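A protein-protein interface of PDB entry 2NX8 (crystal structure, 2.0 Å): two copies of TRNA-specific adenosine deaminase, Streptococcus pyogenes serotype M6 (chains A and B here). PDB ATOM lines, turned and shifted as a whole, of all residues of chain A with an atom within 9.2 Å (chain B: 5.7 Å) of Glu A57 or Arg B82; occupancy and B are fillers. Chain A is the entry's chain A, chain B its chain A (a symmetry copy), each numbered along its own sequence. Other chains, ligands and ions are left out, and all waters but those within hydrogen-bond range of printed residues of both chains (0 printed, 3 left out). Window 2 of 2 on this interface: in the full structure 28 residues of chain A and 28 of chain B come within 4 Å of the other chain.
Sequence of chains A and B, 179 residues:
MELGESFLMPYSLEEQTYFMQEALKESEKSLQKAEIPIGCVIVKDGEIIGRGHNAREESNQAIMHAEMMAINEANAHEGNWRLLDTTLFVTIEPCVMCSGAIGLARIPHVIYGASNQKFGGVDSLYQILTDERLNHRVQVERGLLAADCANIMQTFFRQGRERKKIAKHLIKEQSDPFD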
ATOM      1  N   SER A  30       2.578  22.072 -17.404  1.00  0.00           N
ATOM      2  CA  SER A  30       2.118  20.776 -16.919  1.00  0.00           C
ATOM      3  C   SER A  30       1.503  19.967 -18.064  1.00  0.00           C
ATOM      4  O   SER A  30       1.796  18.778 -18.224  1.00  0.00           O
ATOM      5  CB  SER A  30       1.078  20.958 -15.808  1.00  0.00           C
ATOM      6  OG  SER A  30       1.635  21.626 -14.691  1.00  0.00           O
ATOM      7  N   LYS A  33       3.829  18.295 -20.234  1.00  0.00           N
ATOM      8  CA  LYS A  33       4.492  17.185 -19.560  1.00  0.00           C
ATOM      9  C   LYS A  33       3.505  16.095 -19.168  1.00  0.00           C
ATOM     10  O   LYS A  33       3.805  15.238 -18.339  1.00  0.00           O
ATOM     11  CB  LYS A  33       5.232  17.695 -18.327  1.00  0.00           C
ATOM     12  CG  LYS A  33       6.310  18.717 -18.669  1.00  0.00           C
ATOM     13  CD  LYS A  33       6.883  19.362 -17.425  1.00  0.00           C
ATOM     14  CE  LYS A  33       7.490  18.311 -16.523  1.00  0.00           C
ATOM     15  NZ  LYS A  33       8.521  17.511 -17.249  1.00  0.00           N
ATOM     16  N   ALA A  34       2.325  16.143 -19.773  1.00  0.00           N
ATOM     17  CA  ALA A  34       1.279  15.159 -19.527  1.00  0.00           C
ATOM     18  C   ALA A  34       0.814  15.104 -18.074  1.00  0.00           C
ATOM     19  O   ALA A  34       0.585  14.024 -17.531  1.00  0.00           O
ATOM     20  CB  ALA A  34       1.752  13.783 -19.977  1.00  0.00           C
ATOM     21  N   GLU A  35       0.668  16.267 -17.451  1.00  0.00           N
ATOM     22  CA  GLU A  35       0.208  16.341 -16.068  1.00  0.00           C
ATOM     23  C   GLU A  35      -0.975  17.285 -15.948  1.00  0.00           C
ATOM     24  O   GLU A  35      -1.203  18.112 -16.831  1.00  0.00           O
ATOM     25  CB  GLU A  35       1.349  16.788 -15.159  1.00  0.00           C
ATOM     26  CG  GLU A  35       2.501  15.788 -15.163  1.00  0.00           C
ATOM     27  CD  GLU A  35       3.317  15.820 -13.897  1.00  0.00           C
ATOM     28  OE1 GLU A  35       4.508  16.178 -13.977  1.00  0.00           O
ATOM     29  OE2 GLU A  35       2.762  15.486 -12.826  1.00  0.00           O
ATOM     30  N   ILE A  36      -1.739  17.143 -14.869  1.00  0.00           N
ATOM     31  CA  ILE A  36      -2.908  17.988 -14.645  1.00  0.00           C
ATOM     32  C   ILE A  36      -2.480  19.428 -14.914  1.00  0.00           C
ATOM     33  O   ILE A  36      -1.606  19.959 -14.234  1.00  0.00           O
ATOM     34  CB  ILE A  36      -3.416  17.876 -13.197  1.00  0.00           C
ATOM     35  CG1 ILE A  36      -3.522  16.405 -12.783  1.00  0.00           C
ATOM     36  CG2 ILE A  36      -4.777  18.543 -13.077  1.00  0.00           C
ATOM     37  CD1 ILE A  36      -4.749  15.687 -13.311  1.00  0.00           C
ATOM     38  N   HIS A  53       3.409  25.041 -11.139  1.00  0.00           N
ATOM     39  CA  HIS A  53       2.534  24.237 -11.977  1.00  0.00           C
ATOM     40  C   HIS A  53       2.588  22.824 -11.407  1.00  0.00           C
ATOM     41  O   HIS A  53       3.546  22.473 -10.730  1.00  0.00           O
ATOM     42  CB  HIS A  53       3.014  24.239 -13.434  1.00  0.00           C
ATOM     43  CG  HIS A  53       4.416  23.746 -13.614  1.00  0.00           C
ATOM     44  ND1 HIS A  53       5.521  24.536 -13.382  1.00  0.00           N
ATOM     45  CD2 HIS A  53       4.892  22.535 -13.995  1.00  0.00           C
ATOM     46  CE1 HIS A  53       6.619  23.834 -13.610  1.00  0.00           C
ATOM     47  NE2 HIS A  53       6.264  22.617 -13.984  1.00  0.00           N
ATOM     48  N   ASN A  54       1.559  22.021 -11.655  1.00  0.00           N
ATOM     49  CA  ASN A  54       1.554  20.657 -11.147  1.00  0.00           C
ATOM     50  C   ASN A  54       2.676  19.854 -11.798  1.00  0.00           C
ATOM     51  O   ASN A  54       2.830  19.874 -13.026  1.00  0.00           O
ATOM     52  CB  ASN A  54       0.208  19.976 -11.418  1.00  0.00           C
ATOM     53  CG  ASN A  54      -0.866  20.380 -10.423  1.00  0.00           C
ATOM     54  OD1 ASN A  54      -1.831  19.645 -10.204  1.00  0.00           O
ATOM     55  ND2 ASN A  54      -0.710  21.548  -9.824  1.00  0.00           N
ATOM     56  N   ALA A  55       3.458  19.155 -10.978  1.00  0.00           N
ATOM     57  CA  ALA A  55       4.573  18.349 -11.470  1.00  0.00           C
ATOM     58  C   ALA A  55       4.812  17.114 -10.606  1.00  0.00           C
ATOM     59  O   ALA A  55       5.952  16.718 -10.381  1.00  0.00           O
ATOM     60  CB  ALA A  55       5.838  19.191 -11.525  1.00  0.00           C
ATOM     61  N   ARG A  56       3.725  16.516 -10.137  1.00  0.00           N
ATOM     62  CA  ARG A  56       3.763  15.322  -9.299  1.00  0.00           C
ATOM     63  C   ARG A  56       4.512  14.161  -9.953  1.00  0.00           C
ATOM     64  O   ARG A  56       5.410  13.570  -9.348  1.00  0.00           O
ATOM     65  CB  ARG A  56       2.333  14.877  -8.987  1.00  0.00           C
ATOM     66  CG  ARG A  56       2.227  13.631  -8.133  1.00  0.00           C
ATOM     67  CD  ARG A  56       0.839  13.008  -8.238  1.00  0.00           C
ATOM     68  NE  ARG A  56       0.613  12.374  -9.537  1.00  0.00           N
ATOM     69  CZ  ARG A  56      -0.490  11.705  -9.865  1.00  0.00           C
ATOM     70  NH1 ARG A  56      -0.607  11.158 -11.072  1.00  0.00           N
ATOM     71  NH2 ARG A  56      -1.482  11.582  -8.991  1.00  0.00           N
ATOM     72  N   GLU A  57       4.137  13.828 -11.186  1.00  0.00           N
ATOM     73  CA  GLU A  57       4.769  12.724 -11.895  1.00  0.00           C
ATOM     74  C   GLU A  57       6.235  12.978 -12.194  1.00  0.00           C
ATOM     75  O   GLU A  57       7.075  12.103 -12.000  1.00  0.00           O
ATOM     76  CB  GLU A  57       4.034  12.427 -13.202  1.00  0.00           C
ATOM     77  CG  GLU A  57       2.678  11.757 -13.032  1.00  0.00           C
ATOM     78  CD  GLU A  57       2.764  10.448 -12.269  1.00  0.00           C
ATOM     79  OE1 GLU A  57       3.810   9.768 -12.356  1.00  0.00           O
ATOM     80  OE2 GLU A  57       1.776  10.088 -11.590  1.00  0.00           O
ATOM     81  N   GLU A  58       6.549  14.176 -12.663  1.00  0.00           N
ATOM     82  CA  GLU A  58       7.931  14.503 -12.982  1.00  0.00           C
ATOM     83  C   GLU A  58       8.829  14.540 -11.747  1.00  0.00           C
ATOM     84  O   GLU A  58       9.953  14.045 -11.777  1.00  0.00           O
ATOM     85  CB  GLU A  58       8.013  15.855 -13.694  1.00  0.00           C
ATOM     86  CG  GLU A  58       9.443  16.300 -13.960  1.00  0.00           C
ATOM     87  CD  GLU A  58       9.537  17.745 -14.403  1.00  0.00           C
ATOM     88  OE1 GLU A  58       9.029  18.629 -13.676  1.00  0.00           O
ATOM     89  OE2 GLU A  58      10.121  18.002 -15.477  1.00  0.00           O
ATOM     90  N   SER A  59       8.327  15.130 -10.666  1.00  0.00           N
ATOM     91  CA  SER A  59       9.111  15.264  -9.442  1.00  0.00           C
ATOM     92  C   SER A  59       9.013  14.070  -8.509  1.00  0.00           C
ATOM     93  O   SER A  59       9.823  13.932  -7.594  1.00  0.00           O
ATOM     94  CB  SER A  59       8.685  16.523  -8.679  1.00  0.00           C
ATOM     95  OG  SER A  59       7.384  16.376  -8.127  1.00  0.00           O
ATOM     96  N   ASN A  60       8.026  13.212  -8.737  1.00  0.00           N
ATOM     97  CA  ASN A  60       7.814  12.049  -7.884  1.00  0.00           C
ATOM     98  C   ASN A  60       7.464  12.516  -6.471  1.00  0.00           C
ATOM     99  O   ASN A  60       7.608  11.763  -5.509  1.00  0.00           O
ATOM    100  CB  ASN A  60       9.070  11.167  -7.837  1.00  0.00           C
ATOM    101  CG  ASN A  60       9.367  10.506  -9.169  1.00  0.00           C
ATOM    102  OD1 ASN A  60       8.496   9.880  -9.767  1.00  0.00           O
ATOM    103  ND2 ASN A  60      10.608  10.635  -9.632  1.00  0.00           N
ATOM    104  N   GLN A  61       7.005  13.762  -6.365  1.00  0.00           N
ATOM    105  CA  GLN A  61       6.611  14.369  -5.093  1.00  0.00           C
ATOM    106  C   GLN A  61       5.093  14.529  -5.028  1.00  0.00           C
ATOM    107  O   GLN A  61       4.491  15.197  -5.870  1.00  0.00           O
ATOM    108  CB  GLN A  61       7.276  15.739  -4.930  1.00  0.00           C
ATOM    109  CG  GLN A  61       8.719  15.698  -4.434  1.00  0.00           C
ATOM    110  CD  GLN A  61       9.375  17.074  -4.424  1.00  0.00           C
ATOM    111  OE1 GLN A  61       9.999  17.481  -5.399  1.00  0.00           O
ATOM    112  NE2 GLN A  61       9.222  17.798  -3.323  1.00  0.00           N
ATOM    113  N   ALA A  62       4.484  13.922  -4.014  1.00  0.00           N
ATOM    114  CA  ALA A  62       3.036  13.970  -3.830  1.00  0.00           C
ATOM    115  C   ALA A  62       2.468  15.355  -3.526  1.00  0.00           C
ATOM    116  O   ALA A  62       1.293  15.610  -3.784  1.00  0.00           O
ATOM    117  CB  ALA A  62       2.627  13.004  -2.729  1.00  0.00           C
ATOM    118  N   ILE A  63       3.289  16.246  -2.979  1.00  0.00           N
ATOM    119  CA  ILE A  63       2.830  17.594  -2.626  1.00  0.00           C
ATOM    120  C   ILE A  63       3.100  18.619  -3.717  1.00  0.00           C
ATOM    121  O   ILE A  63       2.775  19.796  -3.547  1.00  0.00           O
ATOM    122  CB  ILE A  63       3.545  18.128  -1.370  1.00  0.00           C
ATOM    123  CG1 ILE A  63       4.983  18.507  -1.727  1.00  0.00           C
ATOM    124  CG2 ILE A  63       3.545  17.069  -0.266  1.00  0.00           C
ATOM    125  CD1 ILE A  63       5.738  19.221  -0.606  1.00  0.00           C
ATOM    126  N   MET A  64       3.680  18.176  -4.829  1.00  0.00           N
ATOM    127  CA  MET A  64       4.047  19.092  -5.899  1.00  0.00           C
ATOM    128  C   MET A  64       2.930  19.637  -6.781  1.00  0.00           C
ATOM    129  O   MET A  64       2.941  19.464  -8.008  1.00  0.00           O
ATOM    130  CB  MET A  64       5.137  18.464  -6.769  1.00  0.00           C
ATOM    131  CG  MET A  64       5.956  19.484  -7.544  1.00  0.00           C
ATOM    132  SD  MET A  64       6.551  20.810  -6.469  1.00  0.00           S
ATOM    133  CE  MET A  64       7.606  19.892  -5.359  1.00  0.00           C
ATOM    134  N   HIS A  65       1.963  20.290  -6.144  1.00  0.00           N
ATOM    135  CA  HIS A  65       0.872  20.925  -6.865  1.00  0.00           C
ATOM    136  C   HIS A  65       1.365  22.322  -7.190  1.00  0.00           C
ATOM    137  O   HIS A  65       2.336  22.795  -6.591  1.00  0.00           O
ATOM    138  CB  HIS A  65      -0.387  21.008  -6.003  1.00  0.00           C
ATOM    139  CG  HIS A  65      -1.174  19.739  -5.967  1.00  0.00           C
ATOM    140  ND1 HIS A  65      -2.428  19.658  -5.404  1.00  0.00           N
ATOM    141  CD2 HIS A  65      -0.896  18.503  -6.444  1.00  0.00           C
ATOM    142  CE1 HIS A  65      -2.891  18.428  -5.536  1.00  0.00           C
ATOM    143  NE2 HIS A  65      -1.980  17.706  -6.164  1.00  0.00           N
ATOM    144  N   PHE A 156      -6.489  18.164 -21.388  1.00  0.00           N
ATOM    145  CA  PHE A 156      -5.688  17.176 -20.678  1.00  0.00           C
ATOM    146  C   PHE A 156      -6.368  15.807 -20.628  1.00  0.00           C
ATOM    147  O   PHE A 156      -5.743  14.790 -20.919  1.00  0.00           O
ATOM    148  CB  PHE A 156      -5.417  17.646 -19.247  1.00  0.00           C
ATOM    149  CG  PHE A 156      -4.800  16.592 -18.374  1.00  0.00           C
ATOM    150  CD1 PHE A 156      -3.495  16.164 -18.593  1.00  0.00           C
ATOM    151  CD2 PHE A 156      -5.529  16.015 -17.344  1.00  0.00           C
ATOM    152  CE1 PHE A 156      -2.922  15.173 -17.793  1.00  0.00           C
ATOM    153  CE2 PHE A 156      -4.969  15.025 -16.540  1.00  0.00           C
ATOM    154  CZ  PHE A 156      -3.664  14.604 -16.765  1.00  0.00           C
ATOM    155  N   ARG A 163      -3.706   8.826 -25.057  1.00  0.00           N
ATOM    156  CA  ARG A 163      -2.454   8.196 -24.650  1.00  0.00           C
ATOM    157  C   ARG A 163      -2.741   6.788 -24.132  1.00  0.00           C
ATOM    158  O   ARG A 163      -1.978   5.857 -24.373  1.00  0.00           O
ATOM    159  CB  ARG A 163      -1.767   9.017 -23.551  1.00  0.00           C
ATOM    160  CG  ARG A 163      -1.344  10.422 -23.974  1.00  0.00           C
ATOM    161  CD  ARG A 163      -0.412  11.065 -22.945  1.00  0.00           C
ATOM    162  NE  ARG A 163      -1.075  11.370 -21.678  1.00  0.00           N
ATOM    163  CZ  ARG A 163      -1.626  12.544 -21.378  1.00  0.00           C
ATOM    164  NH1 ARG A 163      -1.598  13.539 -22.257  1.00  0.00           N
ATOM    165  NH2 ARG A 163      -2.202  12.729 -20.195  1.00  0.00           N
ATOM    166  N   ASN B  75       9.140  10.019  -0.733  1.00  0.00           N
ATOM    167  CA  ASN B  75       8.937   9.987  -2.179  1.00  0.00           C
ATOM    168  C   ASN B  75      10.281   9.829  -2.873  1.00  0.00           C
ATOM    169  O   ASN B  75      10.420   9.048  -3.810  1.00  0.00           O
ATOM    170  CB  ASN B  75       8.268  11.270  -2.686  1.00  0.00           C
ATOM    171  CG  ASN B  75       6.806  11.363  -2.307  1.00  0.00           C
ATOM    172  OD1 ASN B  75       6.077  10.366  -2.317  1.00  0.00           O
ATOM    173  ND2 ASN B  75       6.362  12.566  -1.995  1.00  0.00           N
ATOM    174  N   GLU B  78      11.609   6.231  -2.518  1.00  0.00           N
ATOM    175  CA  GLU B  78      10.875   5.327  -3.399  1.00  0.00           C
ATOM    176  C   GLU B  78      10.885   5.767  -4.859  1.00  0.00           C
ATOM    177  O   GLU B  78      10.530   4.990  -5.742  1.00  0.00           O
ATOM    178  CB  GLU B  78       9.420   5.224  -2.933  1.00  0.00           C
ATOM    179  CG  GLU B  78       9.266   4.677  -1.536  1.00  0.00           C
ATOM    180  CD  GLU B  78       9.713   3.240  -1.443  1.00  0.00           C
ATOM    181  OE1 GLU B  78       9.001   2.360  -1.975  1.00  0.00           O
ATOM    182  OE2 GLU B  78      10.784   2.994  -0.850  1.00  0.00           O
ATOM    183  N   ASN B  80       8.896   7.740  -6.225  1.00  0.00           N
ATOM    184  CA  ASN B  80       7.498   7.634  -6.622  1.00  0.00           C
ATOM    185  C   ASN B  80       6.660   8.502  -5.688  1.00  0.00           C
ATOM    186  O   ASN B  80       6.890   8.514  -4.479  1.00  0.00           O
ATOM    187  CB  ASN B  80       7.064   6.169  -6.516  1.00  0.00           C
ATOM    188  CG  ASN B  80       5.617   5.947  -6.905  1.00  0.00           C
ATOM    189  OD1 ASN B  80       4.902   6.888  -7.250  1.00  0.00           O
ATOM    190  ND2 ASN B  80       5.176   4.691  -6.849  1.00  0.00           N
ATOM    191  N   TRP B  81       5.693   9.230  -6.240  1.00  0.00           N
ATOM    192  CA  TRP B  81       4.849  10.081  -5.411  1.00  0.00           C
ATOM    193  C   TRP B  81       3.866   9.233  -4.623  1.00  0.00           C
ATOM    194  O   TRP B  81       3.275   9.701  -3.656  1.00  0.00           O
ATOM    195  CB  TRP B  81       4.076  11.107  -6.262  1.00  0.00           C
ATOM    196  CG  TRP B  81       3.066  10.505  -7.194  1.00  0.00           C
ATOM    197  CD1 TRP B  81       3.252  10.188  -8.508  1.00  0.00           C
ATOM    198  CD2 TRP B  81       1.727  10.104  -6.870  1.00  0.00           C
ATOM    199  NE1 TRP B  81       2.114   9.611  -9.022  1.00  0.00           N
ATOM    200  CE2 TRP B  81       1.164   9.546  -8.039  1.00  0.00           C
ATOM    201  CE3 TRP B  81       0.950  10.160  -5.704  1.00  0.00           C
ATOM    202  CZ2 TRP B  81      -0.146   9.043  -8.077  1.00  0.00           C
ATOM    203  CZ3 TRP B  81      -0.352   9.662  -5.742  1.00  0.00           C
ATOM    204  CH2 TRP B  81      -0.884   9.110  -6.921  1.00  0.00           C
ATOM    205  N   ARG B  82       3.685   7.987  -5.045  1.00  0.00           N
ATOM    206  CA  ARG B  82       2.769   7.080  -4.368  1.00  0.00           C
ATOM    207  C   ARG B  82       3.494   6.424  -3.200  1.00  0.00           C
ATOM    208  O   ARG B  82       4.606   5.919  -3.355  1.00  0.00           O
ATOM    209  CB  ARG B  82       2.271   5.996  -5.328  1.00  0.00           C
ATOM    210  CG  ARG B  82       1.661   6.510  -6.625  1.00  0.00           C
ATOM    211  CD  ARG B  82       1.330   5.347  -7.565  1.00  0.00           C
ATOM    212  NE  ARG B  82       0.828   5.782  -8.870  1.00  0.00           N
ATOM    213  CZ  ARG B  82       1.543   6.460  -9.765  1.00  0.00           C
ATOM    214  NH1 ARG B  82       2.802   6.791  -9.506  1.00  0.00           N
ATOM    215  NH2 ARG B  82       1.002   6.800 -10.931  1.00  0.00           N
ATOM    216  N   LEU B  83       2.860   6.441  -2.033  1.00  0.00           N
ATOM    217  CA  LEU B  83       3.438   5.850  -0.830  1.00  0.00           C
ATOM    218  C   LEU B  83       2.493   4.787  -0.276  1.00  0.00           C
ATOM    219  O   LEU B  83       2.057   4.865   0.866  1.00  0.00           O
ATOM    220  CB  LEU B  83       3.689   6.945   0.214  1.00  0.00           C
ATOM    221  CG  LEU B  83       5.078   7.591   0.308  1.00  0.00           C
ATOM    222  CD1 LEU B  83       5.810   7.530  -1.008  1.00  0.00           C
ATOM    223  CD2 LEU B  83       4.927   9.022   0.793  1.00  0.00           C
ATOM    224  N   LEU B  84       2.181   3.795  -1.103  1.00  0.00           N
ATOM    225  CA  LEU B  84       1.287   2.708  -0.716  1.00  0.00           C
ATOM    226  C   LEU B  84       1.972   1.780   0.296  1.00  0.00           C
ATOM    227  O   LEU B  84       3.197   1.733   0.364  1.00  0.00           O
ATOM    228  CB  LEU B  84       0.887   1.917  -1.966  1.00  0.00           C
ATOM    229  CG  LEU B  84       0.196   2.728  -3.071  1.00  0.00           C
ATOM    230  CD1 LEU B  84       0.209   1.950  -4.376  1.00  0.00           C
ATOM    231  CD2 LEU B  84      -1.236   3.051  -2.648  1.00  0.00           C
ATOM    232  N   ALA B 105      -0.591  11.377  -1.017  1.00  0.00           N
ATOM    233  CA  ALA B 105       0.511  10.413  -1.082  1.00  0.00           C
ATOM    234  C   ALA B 105      -0.003   8.978  -1.045  1.00  0.00           C
ATOM    235  O   ALA B 105       0.755   8.026  -1.249  1.00  0.00           O
ATOM    236  CB  ALA B 105       1.484  10.644   0.080  1.00  0.00           C
ATOM    237  N   ARG B 106      -1.295   8.838  -0.778  1.00  0.00           N
ATOM    238  CA  ARG B 106      -1.935   7.538  -0.707  1.00  0.00           C
ATOM    239  C   ARG B 106      -1.435   6.696   0.465  1.00  0.00           C
ATOM    240  O   ARG B 106      -1.447   5.469   0.406  1.00  0.00           O
ATOM    241  CB  ARG B 106      -1.756   6.782  -2.032  1.00  0.00           C
ATOM    242  CG  ARG B 106      -2.427   7.483  -3.212  1.00  0.00           C
ATOM    243  CD  ARG B 106      -3.898   7.732  -2.902  1.00  0.00           C
ATOM    244  NE  ARG B 106      -4.365   9.033  -3.385  1.00  0.00           N
ATOM    245  CZ  ARG B 106      -5.476   9.635  -2.961  1.00  0.00           C
ATOM    246  NH1 ARG B 106      -6.240   9.052  -2.041  1.00  0.00           N
ATOM    247  NH2 ARG B 106      -5.818  10.823  -3.447  1.00  0.00           N
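The backbone carbonyl oxygen of Asn A60 sits close to the backbone NH of Trp B81 (3.3 Å). ND2 of Asn B75 sits close to N of Ala A62, 3.1 Å away. The indole nitrogen (NE1) of Trp B81 sits close to the guanidinium group (NE) of Arg A56. NH2 of Arg B82 lies within salt-bridge range of OE2 of Glu A57 (3.4 Å). NE1 of Trp B81 lies within hydrogen-bond range of OE2 of Glu A57 (2.6 Å). O of Asn A60 lies close to O of Asn B80 (3.5 Å).
O of Arg A56 lies within hydrogen-bond range of N of Gln A61, at 3.4 Å. The backbone NH (N) of Leu B83 lies within hydrogen-bond range of the backbone carbonyl oxygen (O) of Ala B105, 2.7 Å away. OD1 of Asn B75 lies close to O of Trp B81 (3.2 Å). The backbone carbonyl oxygen (O) of Asn B80 sits close to the side-chain amide oxygen (OD1) of Asn B75, at 3.0 Å. The side-chain hydroxyl (OG) of Ser A59 lies close to the backbone NH (N) of Gln A61, at 3.2 Å. The side-chain amide oxygen of Asn A60 lies close to the backbone carbonyl oxygen of Glu A57.
Among the printed residues, pairs that only touch across the chains: Asn A60 with Asn B75 (2.9 Å), Gln A61 with Asn B75 (3.6 Å), Gln A61 with Trp B81 (3.8 Å), Ala A62 with Trp B81 (3.5 Å) and Ala A62 with Ala B105 (3.7 Å).
Lys A33 touches none of the printed residues of chain B. Of the printed residues of chain B, Ala A62 touches Asn B75, Trp B81 and Ala B105. Trp B81 touches just these residues of chain A: Arg A56, Glu A57, Asn A60, Gln A61 and Ala A62. Of chain A, only Glu A57 comes within 4 Å of Arg B82. No residue of chain A comes within 4 Å of Leu B83. Printed residues of chain A within 4 Å of Ala B105: Ala A62 (3.7 Å).
Of the 9 printed residues of chain B, 5 touch a printed residue of chain A. Of the 20 printed residues of chain A, 5 touch a printed residue of chain B. Printed residues of chain A that touch a printed residue of chain B: Arg A56, Glu A57, Asn A60, Gln A61 and Ala A62. Hydrophobic or aromatic side chains of chain A within 4 Å of the printed part of chain B: Ala A62. Among the printed residues, Asp or Glu carboxylates within 4 Å of a Lys or Arg side-chain nitrogen of the other chain: Glu A57 with Arg B82.
No position is printed for both chains.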
